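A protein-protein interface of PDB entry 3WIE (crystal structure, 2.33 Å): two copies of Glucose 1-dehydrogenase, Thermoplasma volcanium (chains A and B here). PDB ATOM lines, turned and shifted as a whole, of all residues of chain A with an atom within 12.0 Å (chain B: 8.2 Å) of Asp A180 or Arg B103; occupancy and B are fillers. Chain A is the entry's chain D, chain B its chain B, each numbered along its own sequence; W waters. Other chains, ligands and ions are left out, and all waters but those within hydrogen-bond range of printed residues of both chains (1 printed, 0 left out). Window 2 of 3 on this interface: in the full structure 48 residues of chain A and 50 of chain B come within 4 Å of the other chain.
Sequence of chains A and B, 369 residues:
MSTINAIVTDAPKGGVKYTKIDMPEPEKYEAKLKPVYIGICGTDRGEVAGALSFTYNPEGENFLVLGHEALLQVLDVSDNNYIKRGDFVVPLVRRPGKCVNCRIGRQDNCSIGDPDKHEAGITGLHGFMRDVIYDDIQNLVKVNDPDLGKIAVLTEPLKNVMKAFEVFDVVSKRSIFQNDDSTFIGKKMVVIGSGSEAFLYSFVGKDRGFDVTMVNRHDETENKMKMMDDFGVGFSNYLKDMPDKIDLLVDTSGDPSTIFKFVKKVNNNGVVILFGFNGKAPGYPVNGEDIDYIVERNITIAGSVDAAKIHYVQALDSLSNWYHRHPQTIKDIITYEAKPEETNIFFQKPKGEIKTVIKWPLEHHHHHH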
ATOM      1  N   SER A 175      18.281  26.673 -25.367  1.00  0.00           N
ATOM      2  CA  SER A 175      16.915  26.574 -25.832  1.00  0.00           C
ATOM      3  C   SER A 175      16.229  27.861 -25.403  1.00  0.00           C
ATOM      4  O   SER A 175      16.872  28.703 -24.735  1.00  0.00           O
ATOM      5  CB  SER A 175      16.269  25.357 -25.247  1.00  0.00           C
ATOM      6  OG  SER A 175      15.853  25.685 -23.953  1.00  0.00           O
ATOM      7  N   ILE A 176      14.985  28.077 -25.818  1.00  0.00           N
ATOM      8  CA  ILE A 176      14.286  29.278 -25.351  1.00  0.00           C
ATOM      9  C   ILE A 176      13.653  28.916 -24.027  1.00  0.00           C
ATOM     10  O   ILE A 176      12.749  28.101 -23.971  1.00  0.00           O
ATOM     11  CB  ILE A 176      13.215  29.749 -26.311  1.00  0.00           C
ATOM     12  CG1 ILE A 176      13.847  30.167 -27.629  1.00  0.00           C
ATOM     13  CG2 ILE A 176      12.370  30.886 -25.690  1.00  0.00           C
ATOM     14  CD1 ILE A 176      12.751  30.445 -28.641  1.00  0.00           C
ATOM     15  N   PHE A 177      14.185  29.490 -22.964  1.00  0.00           N
ATOM     16  CA  PHE A 177      13.760  29.180 -21.599  1.00  0.00           C
ATOM     17  C   PHE A 177      12.505  29.976 -21.268  1.00  0.00           C
ATOM     18  O   PHE A 177      11.676  29.507 -20.534  1.00  0.00           O
ATOM     19  CB  PHE A 177      14.897  29.603 -20.628  1.00  0.00           C
ATOM     20  CG  PHE A 177      14.747  29.080 -19.248  1.00  0.00           C
ATOM     21  CD1 PHE A 177      15.166  27.790 -18.925  1.00  0.00           C
ATOM     22  CD2 PHE A 177      14.164  29.893 -18.235  1.00  0.00           C
ATOM     23  CE1 PHE A 177      15.020  27.302 -17.599  1.00  0.00           C
ATOM     24  CE2 PHE A 177      13.992  29.406 -16.933  1.00  0.00           C
ATOM     25  CZ  PHE A 177      14.458  28.122 -16.603  1.00  0.00           C
ATOM     26  N   GLN A 178      12.403  31.171 -21.861  1.00  0.00           N
ATOM     27  CA  GLN A 178      11.340  32.136 -21.535  1.00  0.00           C
ATOM     28  C   GLN A 178      10.014  31.692 -22.057  1.00  0.00           C
ATOM     29  O   GLN A 178       9.939  30.733 -22.848  1.00  0.00           O
ATOM     30  CB  GLN A 178      11.610  33.491 -22.116  1.00  0.00           C
ATOM     31  CG  GLN A 178      12.894  34.068 -21.638  1.00  0.00           C
ATOM     32  CD  GLN A 178      14.080  33.671 -22.528  1.00  0.00           C
ATOM     33  OE1 GLN A 178      14.032  32.691 -23.271  1.00  0.00           O
ATOM     34  NE2 GLN A 178      15.135  34.448 -22.451  1.00  0.00           N
ATOM     35  N   ASN A 179       8.967  32.352 -21.615  1.00  0.00           N
ATOM     36  CA  ASN A 179       7.635  32.167 -22.130  1.00  0.00           C
ATOM     37  C   ASN A 179       7.574  32.810 -23.485  1.00  0.00           C
ATOM     38  O   ASN A 179       8.434  33.575 -23.833  1.00  0.00           O
ATOM     39  CB  ASN A 179       6.582  32.844 -21.272  1.00  0.00           C
ATOM     40  CG  ASN A 179       6.520  32.345 -19.865  1.00  0.00           C
ATOM     41  OD1 ASN A 179       6.244  31.201 -19.595  1.00  0.00           O
ATOM     42  ND2 ASN A 179       6.709  33.250 -18.955  1.00  0.00           N
ATOM     43  N   ASP A 180       6.528  32.507 -24.232  1.00  0.00           N
ATOM     44  CA  ASP A 180       6.342  33.077 -25.552  1.00  0.00           C
ATOM     45  C   ASP A 180       6.020  34.556 -25.568  1.00  0.00           C
ATOM     46  O   ASP A 180       5.933  35.135 -26.604  1.00  0.00           O
ATOM     47  CB  ASP A 180       5.449  32.241 -26.462  1.00  0.00           C
ATOM     48  CG  ASP A 180       4.024  32.238 -26.057  1.00  0.00           C
ATOM     49  OD1 ASP A 180       3.713  32.636 -24.955  1.00  0.00           O
ATOM     50  OD2 ASP A 180       3.199  31.812 -26.848  1.00  0.00           O
ATOM     51  N   ASP A 181       5.915  35.185 -24.409  1.00  0.00           N
ATOM     52  CA  ASP A 181       5.867  36.649 -24.339  1.00  0.00           C
ATOM     53  C   ASP A 181       7.202  37.289 -24.139  1.00  0.00           C
ATOM     54  O   ASP A 181       7.293  38.478 -24.142  1.00  0.00           O
ATOM     55  CB  ASP A 181       4.776  37.217 -23.408  1.00  0.00           C
ATOM     56  CG  ASP A 181       4.960  36.863 -21.937  1.00  0.00           C
ATOM     57  OD1 ASP A 181       5.994  36.374 -21.515  1.00  0.00           O
ATOM     58  OD2 ASP A 181       4.028  37.056 -21.196  1.00  0.00           O
ATOM     59  N   SER A 182       8.231  36.459 -24.026  1.00  0.00           N
ATOM     60  CA  SER A 182       9.613  36.840 -23.789  1.00  0.00           C
ATOM     61  C   SER A 182      10.014  36.995 -22.331  1.00  0.00           C
ATOM     62  O   SER A 182      11.144  37.246 -22.045  1.00  0.00           O
ATOM     63  CB  SER A 182       9.973  38.086 -24.560  1.00  0.00           C
ATOM     64  OG  SER A 182       9.571  39.245 -23.906  1.00  0.00           O
ATOM     65  N   THR A 183       9.075  36.810 -21.429  1.00  0.00           N
ATOM     66  CA  THR A 183       9.257  37.042 -20.014  1.00  0.00           C
ATOM     67  C   THR A 183       9.525  35.781 -19.238  1.00  0.00           C
ATOM     68  O   THR A 183       9.388  34.722 -19.746  1.00  0.00           O
ATOM     69  CB  THR A 183       8.047  37.766 -19.376  1.00  0.00           C
ATOM     70  OG1 THR A 183       7.005  36.848 -19.106  1.00  0.00           O
ATOM     71  CG2 THR A 183       7.521  38.819 -20.254  1.00  0.00           C
ATOM     72  N   PHE A 184       9.899  35.931 -17.977  1.00  0.00           N
ATOM     73  CA  PHE A 184      10.028  34.798 -17.060  1.00  0.00           C
ATOM     74  C   PHE A 184       8.843  34.665 -16.175  1.00  0.00           C
ATOM     75  O   PHE A 184       8.871  33.879 -15.260  1.00  0.00           O
ATOM     76  CB  PHE A 184      11.276  34.950 -16.185  1.00  0.00           C
ATOM     77  CG  PHE A 184      12.554  34.746 -16.916  1.00  0.00           C
ATOM     78  CD1 PHE A 184      13.133  35.791 -17.644  1.00  0.00           C
ATOM     79  CD2 PHE A 184      13.191  33.547 -16.888  1.00  0.00           C
ATOM     80  CE1 PHE A 184      14.365  35.629 -18.277  1.00  0.00           C
ATOM     81  CE2 PHE A 184      14.414  33.366 -17.540  1.00  0.00           C
ATOM     82  CZ  PHE A 184      15.009  34.400 -18.223  1.00  0.00           C
ATOM     83  N   ILE A 185       7.775  35.410 -16.459  1.00  0.00           N
ATOM     84  CA  ILE A 185       6.573  35.378 -15.613  1.00  0.00           C
ATOM     85  C   ILE A 185       6.034  33.988 -15.386  1.00  0.00           C
ATOM     86  O   ILE A 185       5.666  33.314 -16.311  1.00  0.00           O
ATOM     87  CB  ILE A 185       5.410  36.206 -16.213  1.00  0.00           C
ATOM     88  CG1 ILE A 185       5.765  37.665 -16.225  1.00  0.00           C
ATOM     89  CG2 ILE A 185       4.107  35.989 -15.435  1.00  0.00           C
ATOM     90  CD1 ILE A 185       4.872  38.464 -17.122  1.00  0.00           C
ATOM     91  N   GLY A 186       5.857  33.606 -14.122  1.00  0.00           N
ATOM     92  CA  GLY A 186       5.347  32.260 -13.778  1.00  0.00           C
ATOM     93  C   GLY A 186       6.384  31.152 -13.827  1.00  0.00           C
ATOM     94  O   GLY A 186       6.051  30.022 -13.545  1.00  0.00           O
ATOM     95  N   LYS A 187       7.631  31.424 -14.239  1.00  0.00           N
ATOM     96  CA  LYS A 187       8.656  30.380 -14.184  1.00  0.00           C
ATOM     97  C   LYS A 187       9.018  30.136 -12.707  1.00  0.00           C
ATOM     98  O   LYS A 187       9.176  31.049 -11.910  1.00  0.00           O
ATOM     99  CB  LYS A 187       9.891  30.751 -15.017  1.00  0.00           C
ATOM    100  CG  LYS A 187       9.600  30.915 -16.509  1.00  0.00           C
ATOM    101  CD  LYS A 187       9.388  29.563 -17.170  1.00  0.00           C
ATOM    102  CE  LYS A 187       9.145  29.712 -18.675  1.00  0.00           C
ATOM    103  NZ  LYS A 187       9.080  28.343 -19.302  1.00  0.00           N
ATOM    104  N   ASP A 247      11.523  24.934 -12.856  1.00  0.00           N
ATOM    105  CA  ASP A 247      12.272  25.430 -14.012  1.00  0.00           C
ATOM    106  C   ASP A 247      13.728  25.742 -13.661  1.00  0.00           C
ATOM    107  O   ASP A 247      14.619  25.538 -14.486  1.00  0.00           O
ATOM    108  CB  ASP A 247      11.549  26.628 -14.639  1.00  0.00           C
ATOM    109  CG  ASP A 247      10.169  26.230 -15.202  1.00  0.00           C
ATOM    110  OD1 ASP A 247      10.086  25.275 -16.017  1.00  0.00           O
ATOM    111  OD2 ASP A 247       9.141  26.852 -14.818  1.00  0.00           O
ATOM    112  N   ASN A 269      13.975  21.447 -20.283  1.00  0.00           N
ATOM    113  CA  ASN A 269      14.861  22.603 -20.429  1.00  0.00           C
ATOM    114  C   ASN A 269      15.185  23.243 -19.112  1.00  0.00           C
ATOM    115  O   ASN A 269      15.672  24.336 -19.080  1.00  0.00           O
ATOM    116  CB  ASN A 269      14.257  23.651 -21.364  1.00  0.00           C
ATOM    117  CG  ASN A 269      13.919  23.082 -22.719  1.00  0.00           C
ATOM    118  OD1 ASN A 269      14.570  22.136 -23.175  1.00  0.00           O
ATOM    119  ND2 ASN A 269      12.896  23.624 -23.358  1.00  0.00           N
ATOM    120  N   PRO B  96       7.046  19.034 -34.856  1.00  0.00           N
ATOM    121  CA  PRO B  96       6.718  20.071 -33.893  1.00  0.00           C
ATOM    122  C   PRO B  96       5.263  20.074 -33.377  1.00  0.00           C
ATOM    123  O   PRO B  96       4.328  19.739 -34.084  1.00  0.00           O
ATOM    124  CB  PRO B  96       6.929  21.345 -34.675  1.00  0.00           C
ATOM    125  CG  PRO B  96       6.761  20.948 -36.123  1.00  0.00           C
ATOM    126  CD  PRO B  96       7.218  19.573 -36.226  1.00  0.00           C
ATOM    127  N   GLY B  97       5.115  20.503 -32.138  1.00  0.00           N
ATOM    128  CA  GLY B  97       3.869  20.905 -31.605  1.00  0.00           C
ATOM    129  C   GLY B  97       3.700  22.394 -31.723  1.00  0.00           C
ATOM    130  O   GLY B  97       3.930  22.992 -32.782  1.00  0.00           O
ATOM    131  N   LYS B  98       3.262  22.992 -30.619  1.00  0.00           N
ATOM    132  CA  LYS B  98       2.854  24.417 -30.587  1.00  0.00           C
ATOM    133  C   LYS B  98       3.676  25.277 -29.602  1.00  0.00           C
ATOM    134  O   LYS B  98       3.547  26.491 -29.610  1.00  0.00           O
ATOM    135  CB  LYS B  98       1.360  24.446 -30.166  1.00  0.00           C
ATOM    136  CG  LYS B  98       0.384  24.522 -31.336  1.00  0.00           C
ATOM    137  CD  LYS B  98       0.362  23.319 -32.266  1.00  0.00           C
ATOM    138  CE  LYS B  98      -0.255  23.657 -33.627  1.00  0.00           C
ATOM    139  NZ  LYS B  98      -0.187  22.455 -34.510  1.00  0.00           N
ATOM    140  N   CYS B  99       4.396  24.642 -28.675  1.00  0.00           N
ATOM    141  CA  CYS B  99       5.193  25.388 -27.671  1.00  0.00           C
ATOM    142  C   CYS B  99       6.191  26.326 -28.342  1.00  0.00           C
ATOM    143  O   CYS B  99       6.404  26.263 -29.567  1.00  0.00           O
ATOM    144  CB  CYS B  99       5.948  24.474 -26.692  1.00  0.00           C
ATOM    145  SG  CYS B  99       7.436  23.637 -27.388  1.00  0.00           S
ATOM    146  N   VAL B 100       6.785  27.192 -27.528  1.00  0.00           N
ATOM    147  CA  VAL B 100       7.622  28.257 -27.992  1.00  0.00           C
ATOM    148  C   VAL B 100       8.901  27.745 -28.759  1.00  0.00           C
ATOM    149  O   VAL B 100       9.352  28.433 -29.702  1.00  0.00           O
ATOM    150  CB  VAL B 100       7.962  29.235 -26.833  1.00  0.00           C
ATOM    151  CG1 VAL B 100       8.816  28.581 -25.762  1.00  0.00           C
ATOM    152  CG2 VAL B 100       8.636  30.530 -27.321  1.00  0.00           C
ATOM    153  N   ASN B 101       9.456  26.589 -28.362  1.00  0.00           N
ATOM    154  CA  ASN B 101      10.550  25.930 -29.111  1.00  0.00           C
ATOM    155  C   ASN B 101      10.117  25.154 -30.378  1.00  0.00           C
ATOM    156  O   ASN B 101      10.800  25.250 -31.400  1.00  0.00           O
ATOM    157  CB  ASN B 101      11.394  25.026 -28.191  1.00  0.00           C
ATOM    158  CG  ASN B 101      12.271  25.857 -27.204  1.00  0.00           C
ATOM    159  OD1 ASN B 101      13.276  26.388 -27.582  1.00  0.00           O
ATOM    160  ND2 ASN B 101      11.791  26.057 -26.010  1.00  0.00           N
ATOM    161  N   CYS B 102       9.004  24.413 -30.309  1.00  0.00           N
ATOM    162  CA  CYS B 102       8.432  23.730 -31.462  1.00  0.00           C
ATOM    163  C   CYS B 102       8.161  24.615 -32.655  1.00  0.00           C
ATOM    164  O   CYS B 102       8.404  24.249 -33.803  1.00  0.00           O
ATOM    165  CB  CYS B 102       7.148  22.978 -31.080  1.00  0.00           C
ATOM    166  SG  CYS B 102       7.544  21.420 -30.323  1.00  0.00           S
ATOM    167  N   ARG B 103       7.748  25.819 -32.392  1.00  0.00           N
ATOM    168  CA  ARG B 103       7.279  26.642 -33.447  1.00  0.00           C
ATOM    169  C   ARG B 103       8.316  27.431 -34.156  1.00  0.00           C
ATOM    170  O   ARG B 103       7.986  28.103 -35.126  1.00  0.00           O
ATOM    171  CB  ARG B 103       6.174  27.540 -32.891  1.00  0.00           C
ATOM    172  CG  ARG B 103       6.571  28.741 -32.020  1.00  0.00           C
ATOM    173  CD  ARG B 103       5.494  28.698 -30.952  1.00  0.00           C
ATOM    174  NE  ARG B 103       5.056  29.952 -30.523  1.00  0.00           N
ATOM    175  CZ  ARG B 103       4.257  30.140 -29.474  1.00  0.00           C
ATOM    176  NH1 ARG B 103       3.783  29.130 -28.775  1.00  0.00           N
ATOM    177  NH2 ARG B 103       3.931  31.370 -29.164  1.00  0.00           N
ATOM    178  N   ILE B 104       9.543  27.429 -33.628  1.00  0.00           N
ATOM    179  CA  ILE B 104      10.731  27.892 -34.349  1.00  0.00           C
ATOM    180  C   ILE B 104      11.523  26.732 -34.973  1.00  0.00           C
ATOM    181  O   ILE B 104      12.612  26.961 -35.475  1.00  0.00           O
ATOM    182  CB  ILE B 104      11.656  28.781 -33.491  1.00  0.00           C
ATOM    183  CG1 ILE B 104      12.282  28.004 -32.326  1.00  0.00           C
ATOM    184  CG2 ILE B 104      10.897  30.031 -33.019  1.00  0.00           C
ATOM    185  CD1 ILE B 104      13.473  28.760 -31.749  1.00  0.00           C
ATOM    186  N   GLY B 105      11.012  25.521 -34.960  1.00  0.00           N
ATOM    187  CA  GLY B 105      11.760  24.422 -35.508  1.00  0.00           C
ATOM    188  C   GLY B 105      12.788  23.835 -34.592  1.00  0.00           C
ATOM    189  O   GLY B 105      13.749  23.245 -35.012  1.00  0.00           O
ATOM    190  N   ARG B 106      12.567  24.052 -33.316  1.00  0.00           N
ATOM    191  CA  ARG B 106      13.395  23.517 -32.288  1.00  0.00           C
ATOM    192  C   ARG B 106      12.600  22.596 -31.427  1.00  0.00           C
ATOM    193  O   ARG B 106      12.688  22.657 -30.232  1.00  0.00           O
ATOM    194  CB  ARG B 106      14.120  24.599 -31.509  1.00  0.00           C
ATOM    195  CG  ARG B 106      14.984  25.483 -32.374  1.00  0.00           C
ATOM    196  CD  ARG B 106      16.139  24.776 -33.056  1.00  0.00           C
ATOM    197  NE  ARG B 106      16.803  23.791 -32.212  1.00  0.00           N
ATOM    198  CZ  ARG B 106      18.081  23.824 -31.831  1.00  0.00           C
ATOM    199  NH1 ARG B 106      18.870  24.799 -32.181  1.00  0.00           N
ATOM    200  NH2 ARG B 106      18.553  22.873 -31.079  1.00  0.00           N
ATOM    201  N   GLN B 107      11.783  21.768 -32.060  1.00  0.00           N
ATOM    202  CA  GLN B 107      11.052  20.775 -31.309  1.00  0.00           C
ATOM    203  C   GLN B 107      11.963  19.769 -30.576  1.00  0.00           C
ATOM    204  O   GLN B 107      11.525  18.971 -29.713  1.00  0.00           O
ATOM    205  CB  GLN B 107      10.079  20.039 -32.286  1.00  0.00           C
ATOM    206  CG  GLN B 107      10.770  19.272 -33.425  1.00  0.00           C
ATOM    207  CD  GLN B 107      10.885  20.110 -34.704  1.00  0.00           C
ATOM    208  OE1 GLN B 107      10.974  21.345 -34.684  1.00  0.00           O
ATOM    209  NE2 GLN B 107      10.815  19.430 -35.824  1.00  0.00           N
ATOM    210  N   CYS B 110      11.530  20.833 -27.167  1.00  0.00           N
ATOM    211  CA  CYS B 110      10.143  21.073 -26.823  1.00  0.00           C
ATOM    212  C   CYS B 110      10.055  21.305 -25.280  1.00  0.00           C
ATOM    213  O   CYS B 110      10.509  20.493 -24.465  1.00  0.00           O
ATOM    214  CB  CYS B 110       9.328  19.832 -27.229  1.00  0.00           C
ATOM    215  SG  CYS B 110       7.552  19.897 -26.750  1.00  0.00           S
ATOM    216  N   SER B 111       9.462  22.425 -24.901  1.00  0.00           N
ATOM    217  CA  SER B 111       9.178  22.777 -23.471  1.00  0.00           C
ATOM    218  C   SER B 111       8.102  21.953 -22.813  1.00  0.00           C
ATOM    219  O   SER B 111       7.973  21.994 -21.585  1.00  0.00           O
ATOM    220  CB  SER B 111       8.667  24.192 -23.408  1.00  0.00           C
ATOM    221  OG  SER B 111       9.435  24.980 -24.299  1.00  0.00           O
ATOM    222  N   ILE B 112       7.368  21.141 -23.579  1.00  0.00           N
ATOM    223  CA  ILE B 112       6.278  20.338 -22.986  1.00  0.00           C
ATOM    224  C   ILE B 112       6.581  18.863 -22.926  1.00  0.00           C
ATOM    225  O   ILE B 112       6.207  18.183 -21.973  1.00  0.00           O
ATOM    226  CB  ILE B 112       4.946  20.582 -23.731  1.00  0.00           C
ATOM    227  CG1 ILE B 112       4.496  22.018 -23.480  1.00  0.00           C
ATOM    228  CG2 ILE B 112       3.872  19.575 -23.275  1.00  0.00           C
ATOM    229  CD1 ILE B 112       3.501  22.500 -24.519  1.00  0.00           C
ATOM    230  N   ASP B 116       2.980  17.336 -26.927  1.00  0.00           N
ATOM    231  CA  ASP B 116       3.220  18.447 -27.869  1.00  0.00           C
ATOM    232  C   ASP B 116       4.037  17.994 -29.125  1.00  0.00           C
ATOM    233  O   ASP B 116       3.623  18.141 -30.249  1.00  0.00           O
ATOM    234  CB  ASP B 116       3.967  19.597 -27.184  1.00  0.00           C
ATOM    235  CG  ASP B 116       3.787  20.918 -27.943  1.00  0.00           C
ATOM    236  OD1 ASP B 116       2.713  21.078 -28.538  1.00  0.00           O
ATOM    237  OD2 ASP B 116       4.672  21.792 -27.987  1.00  0.00           O
HETATM  238  O   HOH W   1      13.322  19.740 -23.981  1.00  0.00           O
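SG of Cys B99 sits close to N of Ser B111 (3.4 Å).
The side-chain hydroxyl (OG) of Ser B111 is in hydrogen-bond range of the side-chain amide nitrogen (ND2) of Asn B101 (3.1 Å).
The backbone NH (N) of Arg B106 lies within hydrogen-bond range of the backbone carbonyl oxygen (O) of Asn B101 (2.9 Å).
The backbone carbonyl oxygen (O) of Lys B98 is in hydrogen-bond range of the guanidinium group (NH1) of Arg B103 (2.8 Å).
The side-chain sulfur of Cys B99 sits close to the backbone NH of Asn B101 (3.7 Å).
The side-chain amide oxygen (OD1) of Asn B101 is in hydrogen-bond range of the backbone NH (N) of Ile A176 (3.0 Å).
The guanidinium group of Arg B103 lies within salt-bridge range of the side-chain carboxylate of Asp A180, 2.5 Å away.
Water W1 bridges OD1 of Asn A269 (2.8 Å) and O of Cys B110 (3.0 Å).
Hydrophobic or aromatic side chains of chain A that line the printed part of chain B: Ile A176.
Along chain A the printed residues that touch a printed residue of chain B span positions 175 to 269.
Among the printed residues, 8 pairs touch across the chains.
No position is printed for both chains.
Of chain B, only Val B100 (3.7 Å) and Arg B103 (2.5 Å) come within 4 Å of Asp A180.
No residue of chain A comes within 4 Å of Pro B96.
No residue of chain A comes within 4 Å of Gly B97.
Cys B99 touches none of the printed residues of chain A.
Of chain A, only Ser A175, Ile A176 and Asn A269 come within 4 Å of Asn B101.
Of the printed residues of chain B, Ile A176 touches Asn B101 and Ile B104.
Printed residues of chain B within 4 Å of Ser A175: Asn B101 (3.9 Å).
Asp A247 touches none of the printed residues of chain B.
Among the printed residues, merely in contact across the chains: Ser A175 with Asn B101 (3.9 Å), Ile A176 with Ile B104 (3.6 Å), Gln A178 with Val B100 (3.8 Å), Asp A180 with Val B100 (3.7 Å), Asn A269 with Asn B101 (3.8 Å) and Asn A269 with Ser B111 (3.8 Å).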
